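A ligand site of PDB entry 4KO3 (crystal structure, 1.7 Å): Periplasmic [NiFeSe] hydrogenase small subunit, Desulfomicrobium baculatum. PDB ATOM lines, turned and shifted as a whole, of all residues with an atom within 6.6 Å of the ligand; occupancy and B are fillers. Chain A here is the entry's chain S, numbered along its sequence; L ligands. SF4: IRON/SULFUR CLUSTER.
A ring nitrogen (ND1) of His 208 is bound to an iron atom (FE3) of the ligand (2.1 Å). SG of Cys 231 is bound to FE1 of the ligand. The side-chain sulfur (SG) of Cys 211 is bound to an iron atom (FE2) of the ligand (2.3 Å). SG of Cys 237 is bound to FE4 of the ligand, at 2.3 Å. The backbone NH (N) of Lys 232 lies close to a sulfur (S3) of the ligand (3.3 Å). N of Leu 214 sits close to S4 of the ligand (3.7 Å).
The backbone carbonyl oxygen (O) of Gly 239 sits at hydrogen-bond distance from the backbone NH (N) of His 208 (3.2 Å). The side-chain sulfur (SG) of Cys 231 lies close to the backbone NH (N) of Ala 233, at 3.3 Å. The side-chain sulfur (SG) of Cys 211 lies close to the backbone NH (N) of Tyr 213. The backbone NH (N) of Cys 237 sits at hydrogen-bond distance from the backbone carbonyl oxygen (O) of Lys 232 (3.4 Å). SG of Cys 237 sits close to N of Gly 239. The backbone NH of Cys 264 sits close to the side-chain sulfur of Cys 237 (3.8 Å). NZ of Lys 232 lies within hydrogen-bond range of O of Val 259 (2.7 Å). NZ of Lys 232 is in hydrogen-bond range of O of Ala 262.
The backbone carbonyl oxygen (O) of Tyr 213 lies close to a sulfur (S4) of the ligand (3.8 Å). Residues that only touch the ligand: Ile 207 (3.99 Å), Tyr 217 (3.9 Å), Ala 233 (3.7 Å), Gly 239 (3.7 Å), Pro 240 (3.9 Å) and Val 259 (3.5 Å). Hydrophobic or aromatic side chains that line the ligand: Ile 207, His 208, Tyr 213, Tyr 217, Ala 233, Pro 240 and Val 259. Within 4 Å of the ligand: Ile 207, His 208, Cys 211, Tyr 213, Leu 214, Tyr 217, Cys 231, Lys 232, Ala 233, Cys 237, Gly 239, Pro 240 and Val 259.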
ATOM      1  N   ILE A 207     -23.443  28.071  11.309  1.00  0.00           N
ATOM      2  CA  ILE A 207     -23.441  28.512   9.909  1.00  0.00           C
ATOM      3  C   ILE A 207     -24.337  27.617   9.043  1.00  0.00           C
ATOM      4  O   ILE A 207     -25.246  28.114   8.369  1.00  0.00           O
ATOM      5  CB  ILE A 207     -22.002  28.539   9.354  1.00  0.00           C
ATOM      6  CG1 ILE A 207     -21.151  29.574  10.120  1.00  0.00           C
ATOM      7  CG2 ILE A 207     -21.997  28.711   7.811  1.00  0.00           C
ATOM      8  CD1 ILE A 207     -20.919  30.898   9.432  1.00  0.00           C
ATOM      9  N   HIS A 208     -24.090  26.311   9.079  1.00  0.00           N
ATOM     10  CA  HIS A 208     -24.827  25.327   8.287  1.00  0.00           C
ATOM     11  C   HIS A 208     -26.355  25.381   8.530  1.00  0.00           C
ATOM     12  O   HIS A 208     -27.143  25.451   7.578  1.00  0.00           O
ATOM     13  CB  HIS A 208     -24.217  23.954   8.562  1.00  0.00           C
ATOM     14  CG  HIS A 208     -24.883  22.814   7.865  1.00  0.00           C
ATOM     15  ND1 HIS A 208     -24.710  22.540   6.526  1.00  0.00           N
ATOM     16  CD2 HIS A 208     -25.700  21.840   8.344  1.00  0.00           C
ATOM     17  CE1 HIS A 208     -25.402  21.456   6.210  1.00  0.00           C
ATOM     18  NE2 HIS A 208     -26.005  21.013   7.296  1.00  0.00           N
ATOM     19  N   GLU A 209     -26.766  25.390   9.795  1.00  0.00           N
ATOM     20  CA  GLU A 209     -28.202  25.435  10.116  1.00  0.00           C
ATOM     21  C   GLU A 209     -28.877  26.667   9.518  1.00  0.00           C
ATOM     22  O   GLU A 209     -30.073  26.647   9.211  1.00  0.00           O
ATOM     23  CB  GLU A 209     -28.442  25.370  11.629  1.00  0.00           C
ATOM     24  CG  GLU A 209     -28.002  24.043  12.255  1.00  0.00           C
ATOM     25  CD  GLU A 209     -28.159  24.021  13.777  1.00  0.00           C
ATOM     26  OE1 GLU A 209     -28.818  24.917  14.355  1.00  0.00           O
ATOM     27  OE2 GLU A 209     -27.591  23.105  14.395  1.00  0.00           O
ATOM     28  N   CYS A 211     -27.719  28.312   6.715  1.00  0.00           N
ATOM     29  CA  CYS A 211     -27.144  28.528   5.389  1.00  0.00           C
ATOM     30  C   CYS A 211     -28.205  28.498   4.286  1.00  0.00           C
ATOM     31  O   CYS A 211     -29.084  27.631   4.285  1.00  0.00           O
ATOM     32  CB  CYS A 211     -26.079  27.476   5.090  1.00  0.00           C
ATOM     33  SG  CYS A 211     -25.247  27.704   3.511  1.00  0.00           S
ATOM     34  N   PRO A 212     -28.127  29.447   3.320  1.00  0.00           N
ATOM     35  CA  PRO A 212     -29.081  29.429   2.204  1.00  0.00           C
ATOM     36  C   PRO A 212     -28.947  28.214   1.271  1.00  0.00           C
ATOM     37  O   PRO A 212     -29.847  27.954   0.458  1.00  0.00           O
ATOM     38  CB  PRO A 212     -28.786  30.724   1.453  1.00  0.00           C
ATOM     39  CG  PRO A 212     -27.381  31.096   1.837  1.00  0.00           C
ATOM     40  CD  PRO A 212     -27.192  30.586   3.242  1.00  0.00           C
ATOM     41  N   TYR A 213     -27.849  27.466   1.389  1.00  0.00           N
ATOM     42  CA  TYR A 213     -27.648  26.250   0.593  1.00  0.00           C
ATOM     43  C   TYR A 213     -28.199  25.000   1.273  1.00  0.00           C
ATOM     44  O   TYR A 213     -28.057  23.900   0.744  1.00  0.00           O
ATOM     45  CB  TYR A 213     -26.159  26.011   0.296  1.00  0.00           C
ATOM     46  CG  TYR A 213     -25.514  27.003  -0.644  1.00  0.00           C
ATOM     47  CD1 TYR A 213     -24.987  28.201  -0.158  1.00  0.00           C
ATOM     48  CD2 TYR A 213     -25.403  26.726  -2.015  1.00  0.00           C
ATOM     49  CE1 TYR A 213     -24.394  29.126  -1.024  1.00  0.00           C
ATOM     50  CE2 TYR A 213     -24.788  27.648  -2.890  1.00  0.00           C
ATOM     51  CZ  TYR A 213     -24.288  28.843  -2.383  1.00  0.00           C
ATOM     52  OH  TYR A 213     -23.696  29.760  -3.204  1.00  0.00           O
ATOM     53  N   LEU A 214     -28.815  25.163   2.452  1.00  0.00           N
ATOM     54  CA  LEU A 214     -29.257  23.994   3.223  1.00  0.00           C
ATOM     55  C   LEU A 214     -30.257  23.120   2.443  1.00  0.00           C
ATOM     56  O   LEU A 214     -30.205  21.893   2.534  1.00  0.00           O
ATOM     57  CB  LEU A 214     -29.791  24.368   4.607  1.00  0.00           C
ATOM     58  CG  LEU A 214     -30.016  23.220   5.595  1.00  0.00           C
ATOM     59  CD1 LEU A 214     -28.709  22.494   5.919  1.00  0.00           C
ATOM     60  CD2 LEU A 214     -30.669  23.730   6.859  1.00  0.00           C
ATOM     61  N   ASP A 215     -31.146  23.751   1.672  1.00  0.00           N
ATOM     62  CA  ASP A 215     -32.090  22.986   0.846  1.00  0.00           C
ATOM     63  C   ASP A 215     -31.356  22.099  -0.165  1.00  0.00           C
ATOM     64  O   ASP A 215     -31.738  20.943  -0.410  1.00  0.00           O
ATOM     65  CB  ASP A 215     -33.114  23.917   0.153  1.00  0.00           C
ATOM     66  CG  ASP A 215     -32.465  24.929  -0.825  1.00  0.00           C
ATOM     67  OD1 ASP A 215     -31.253  25.236  -0.718  1.00  0.00           O
ATOM     68  OD2 ASP A 215     -33.198  25.427  -1.697  1.00  0.00           O
ATOM     69  N   LYS A 216     -30.275  22.611  -0.739  1.00  0.00           N
ATOM     70  CA  LYS A 216     -29.474  21.848  -1.696  1.00  0.00           C
ATOM     71  C   LYS A 216     -28.743  20.699  -1.009  1.00  0.00           C
ATOM     72  O   LYS A 216     -28.757  19.562  -1.496  1.00  0.00           O
ATOM     73  CB  LYS A 216     -28.506  22.767  -2.438  1.00  0.00           C
ATOM     74  CG  LYS A 216     -29.214  23.796  -3.317  1.00  0.00           C
ATOM     75  CD  LYS A 216     -28.237  24.724  -4.020  1.00  0.00           C
ATOM     76  CE  LYS A 216     -28.906  26.010  -4.509  1.00  0.00           C
ATOM     77  NZ  LYS A 216     -30.297  25.785  -4.994  1.00  0.00           N
ATOM     78  N   TYR A 217     -28.151  20.990   0.147  1.00  0.00           N
ATOM     79  CA  TYR A 217     -27.537  19.962   0.993  1.00  0.00           C
ATOM     80  C   TYR A 217     -28.535  18.822   1.260  1.00  0.00           C
ATOM     81  O   TYR A 217     -28.201  17.645   1.107  1.00  0.00           O
ATOM     82  CB  TYR A 217     -27.044  20.586   2.311  1.00  0.00           C
ATOM     83  CG  TYR A 217     -26.494  19.594   3.312  1.00  0.00           C
ATOM     84  CD1 TYR A 217     -27.341  18.957   4.215  1.00  0.00           C
ATOM     85  CD2 TYR A 217     -25.127  19.308   3.365  1.00  0.00           C
ATOM     86  CE1 TYR A 217     -26.852  18.031   5.151  1.00  0.00           C
ATOM     87  CE2 TYR A 217     -24.624  18.387   4.300  1.00  0.00           C
ATOM     88  CZ  TYR A 217     -25.498  17.759   5.189  1.00  0.00           C
ATOM     89  OH  TYR A 217     -25.013  16.864   6.105  1.00  0.00           O
ATOM     90  N   PHE A 222     -24.688  18.744  -4.564  1.00  0.00           N
ATOM     91  CA  PHE A 222     -23.381  19.268  -4.180  1.00  0.00           C
ATOM     92  C   PHE A 222     -22.600  19.769  -5.387  1.00  0.00           C
ATOM     93  O   PHE A 222     -22.489  19.092  -6.415  1.00  0.00           O
ATOM     94  CB  PHE A 222     -22.568  18.193  -3.463  1.00  0.00           C
ATOM     95  CG  PHE A 222     -23.232  17.665  -2.234  1.00  0.00           C
ATOM     96  CD1 PHE A 222     -23.329  18.448  -1.073  1.00  0.00           C
ATOM     97  CD2 PHE A 222     -23.796  16.391  -2.222  1.00  0.00           C
ATOM     98  CE1 PHE A 222     -23.958  17.966   0.067  1.00  0.00           C
ATOM     99  CE2 PHE A 222     -24.420  15.890  -1.096  1.00  0.00           C
ATOM    100  CZ  PHE A 222     -24.508  16.691   0.059  1.00  0.00           C
ATOM    101  N   GLY A 230     -24.815  24.144  -6.334  1.00  0.00           N
ATOM    102  CA  GLY A 230     -24.978  23.165  -5.264  1.00  0.00           C
ATOM    103  C   GLY A 230     -24.350  23.593  -3.953  1.00  0.00           C
ATOM    104  O   GLY A 230     -23.590  24.561  -3.893  1.00  0.00           O
ATOM    105  N   CYS A 231     -24.662  22.849  -2.889  1.00  0.00           N
ATOM    106  CA  CYS A 231     -24.018  23.029  -1.601  1.00  0.00           C
ATOM    107  C   CYS A 231     -22.503  22.807  -1.735  1.00  0.00           C
ATOM    108  O   CYS A 231     -22.046  22.028  -2.586  1.00  0.00           O
ATOM    109  CB  CYS A 231     -24.655  22.056  -0.593  1.00  0.00           C
ATOM    110  SG  CYS A 231     -23.676  21.619   0.842  1.00  0.00           S
ATOM    111  N   LYS A 232     -21.731  23.488  -0.895  1.00  0.00           N
ATOM    112  CA  LYS A 232     -20.259  23.474  -0.951  1.00  0.00           C
ATOM    113  C   LYS A 232     -19.598  22.374  -0.113  1.00  0.00           C
ATOM    114  O   LYS A 232     -18.376  22.350  -0.012  1.00  0.00           O
ATOM    115  CB  LYS A 232     -19.714  24.845  -0.512  1.00  0.00           C
ATOM    116  CG  LYS A 232     -20.379  26.051  -1.175  1.00  0.00           C
ATOM    117  CD  LYS A 232     -20.212  26.042  -2.707  1.00  0.00           C
ATOM    118  CE  LYS A 232     -20.617  27.377  -3.324  1.00  0.00           C
ATOM    119  NZ  LYS A 232     -19.597  28.440  -3.113  1.00  0.00           N
ATOM    120  N   ALA A 233     -20.386  21.486   0.496  1.00  0.00           N
ATOM    121  CA  ALA A 233     -19.850  20.488   1.424  1.00  0.00           C
ATOM    122  C   ALA A 233     -18.700  19.652   0.845  1.00  0.00           C
ATOM    123  O   ALA A 233     -17.700  19.415   1.530  1.00  0.00           O
ATOM    124  CB  ALA A 233     -20.959  19.557   1.916  1.00  0.00           C
ATOM    125  N   GLU A 234     -18.844  19.194  -0.396  1.00  0.00           N
ATOM    126  CA  GLU A 234     -17.819  18.341  -1.003  1.00  0.00           C
ATOM    127  C   GLU A 234     -16.540  19.106  -1.353  1.00  0.00           C
ATOM    128  O   GLU A 234     -15.480  18.502  -1.567  1.00  0.00           O
ATOM    129  CB  GLU A 234     -18.354  17.600  -2.241  1.00  0.00           C
ATOM    130  CG  GLU A 234     -19.423  16.566  -1.937  1.00  0.00           C
ATOM    131  CD  GLU A 234     -19.936  15.872  -3.179  1.00  0.00           C
ATOM    132  OE1 GLU A 234     -20.817  15.004  -3.043  1.00  0.00           O
ATOM    133  OE2 GLU A 234     -19.500  16.199  -4.303  1.00  0.00           O
ATOM    134  N   CYS A 237     -16.414  22.725   2.740  1.00  0.00           N
ATOM    135  CA  CYS A 237     -17.117  23.658   3.620  1.00  0.00           C
ATOM    136  C   CYS A 237     -17.185  23.189   5.081  1.00  0.00           C
ATOM    137  O   CYS A 237     -17.647  22.065   5.351  1.00  0.00           O
ATOM    138  CB  CYS A 237     -18.530  23.917   3.091  1.00  0.00           C
ATOM    139  SG  CYS A 237     -19.366  25.275   3.966  1.00  0.00           S
ATOM    140  N   LYS A 238     -16.723  24.046   5.995  1.00  0.00           N
ATOM    141  CA  LYS A 238     -16.759  23.740   7.434  1.00  0.00           C
ATOM    142  C   LYS A 238     -17.945  24.397   8.156  1.00  0.00           C
ATOM    143  O   LYS A 238     -17.999  24.427   9.389  1.00  0.00           O
ATOM    144  CB  LYS A 238     -15.435  24.065   8.127  1.00  0.00           C
ATOM    145  CG  LYS A 238     -14.213  23.412   7.467  1.00  0.00           C
ATOM    146  CD  LYS A 238     -14.375  21.882   7.371  1.00  0.00           C
ATOM    147  CE  LYS A 238     -13.096  21.184   6.916  1.00  0.00           C
ATOM    148  NZ  LYS A 238     -12.539  21.733   5.658  1.00  0.00           N
ATOM    149  N   GLY A 239     -18.907  24.890   7.388  1.00  0.00           N
ATOM    150  CA  GLY A 239     -20.144  25.456   7.971  1.00  0.00           C
ATOM    151  C   GLY A 239     -20.797  24.557   9.006  1.00  0.00           C
ATOM    152  O   GLY A 239     -21.287  25.069  10.019  1.00  0.00           O
ATOM    153  N   PRO A 240     -20.816  23.226   8.773  1.00  0.00           N
ATOM    154  CA  PRO A 240     -21.437  22.326   9.746  1.00  0.00           C
ATOM    155  C   PRO A 240     -20.862  22.400  11.174  1.00  0.00           C
ATOM    156  O   PRO A 240     -21.613  22.175  12.132  1.00  0.00           O
ATOM    157  CB  PRO A 240     -21.210  20.955   9.119  1.00  0.00           C
ATOM    158  CG  PRO A 240     -21.361  21.232   7.665  1.00  0.00           C
ATOM    159  CD  PRO A 240     -20.541  22.507   7.509  1.00  0.00           C
ATOM    160  N   TRP A 257     -19.921  36.658   0.871  1.00  0.00           N
ATOM    161  CA  TRP A 257     -19.411  35.914   2.042  1.00  0.00           C
ATOM    162  C   TRP A 257     -18.754  34.614   1.609  1.00  0.00           C
ATOM    163  O   TRP A 257     -18.891  34.201   0.447  1.00  0.00           O
ATOM    164  CB  TRP A 257     -20.476  35.672   3.117  1.00  0.00           C
ATOM    165  CG  TRP A 257     -21.574  34.704   2.756  1.00  0.00           C
ATOM    166  CD1 TRP A 257     -22.414  34.756   1.672  1.00  0.00           C
ATOM    167  CD2 TRP A 257     -21.999  33.578   3.544  1.00  0.00           C
ATOM    168  NE1 TRP A 257     -23.320  33.723   1.726  1.00  0.00           N
ATOM    169  CE2 TRP A 257     -23.078  32.981   2.850  1.00  0.00           C
ATOM    170  CE3 TRP A 257     -21.561  33.010   4.751  1.00  0.00           C
ATOM    171  CZ2 TRP A 257     -23.747  31.845   3.343  1.00  0.00           C
ATOM    172  CZ3 TRP A 257     -22.217  31.875   5.232  1.00  0.00           C
ATOM    173  CH2 TRP A 257     -23.297  31.296   4.522  1.00  0.00           C
ATOM    174  N   VAL A 259     -19.081  31.369   2.025  1.00  0.00           N
ATOM    175  CA  VAL A 259     -19.834  30.232   1.526  1.00  0.00           C
ATOM    176  C   VAL A 259     -20.373  30.473   0.121  1.00  0.00           C
ATOM    177  O   VAL A 259     -20.248  29.589  -0.733  1.00  0.00           O
ATOM    178  CB  VAL A 259     -20.937  29.796   2.517  1.00  0.00           C
ATOM    179  CG1 VAL A 259     -21.825  28.712   1.903  1.00  0.00           C
ATOM    180  CG2 VAL A 259     -20.297  29.298   3.820  1.00  0.00           C
ATOM    181  N   ALA A 262     -17.109  30.581  -2.066  1.00  0.00           N
ATOM    182  CA  ALA A 262     -16.196  29.437  -2.020  1.00  0.00           C
ATOM    183  C   ALA A 262     -16.618  28.454  -0.931  1.00  0.00           C
ATOM    184  O   ALA A 262     -17.590  27.734  -1.119  1.00  0.00           O
ATOM    185  CB  ALA A 262     -14.734  29.919  -1.819  1.00  0.00           C
ATOM    186  N   VAL A 263     -15.895  28.427   0.195  1.00  0.00           N
ATOM    187  CA  VAL A 263     -16.228  27.570   1.348  1.00  0.00           C
ATOM    188  C   VAL A 263     -15.985  28.346   2.644  1.00  0.00           C
ATOM    189  O   VAL A 263     -15.184  29.294   2.669  1.00  0.00           O
ATOM    190  CB  VAL A 263     -15.373  26.265   1.383  1.00  0.00           C
ATOM    191  CG1 VAL A 263     -15.749  25.291   0.236  1.00  0.00           C
ATOM    192  CG2 VAL A 263     -13.865  26.594   1.361  1.00  0.00           C
ATOM    193  N   CYS A 264     -16.688  27.944   3.704  1.00  0.00           N
ATOM    194  CA  CYS A 264     -16.328  28.355   5.058  1.00  0.00           C
ATOM    195  C   CYS A 264     -15.122  27.523   5.511  1.00  0.00           C
ATOM    196  O   CYS A 264     -15.104  26.306   5.293  1.00  0.00           O
ATOM    197  CB  CYS A 264     -17.514  28.147   6.015  1.00  0.00           C
ATOM    198  SG  CYS A 264     -17.141  28.506   7.766  1.00  0.00           S
HETATM  199 FE1  SF4 L   1     -23.573  23.312   2.358  1.00  0.00          FE
HETATM  200 FE2  SF4 L   1     -24.091  25.727   3.468  1.00  0.00          FE
HETATM  201 FE3  SF4 L   1     -23.745  23.591   5.002  1.00  0.00          FE
HETATM  202 FE4  SF4 L   1     -21.571  24.691   3.714  1.00  0.00          FE
HETATM  203  S1  SF4 L   1     -22.808  25.638   5.403  1.00  0.00           S
HETATM  204  S2  SF4 L   1     -22.056  22.479   3.891  1.00  0.00           S
HETATM  205  S3  SF4 L   1     -22.641  25.305   1.755  1.00  0.00           S
HETATM  206  S4  SF4 L   1     -25.458  23.891   3.496  1.00  0.00           S
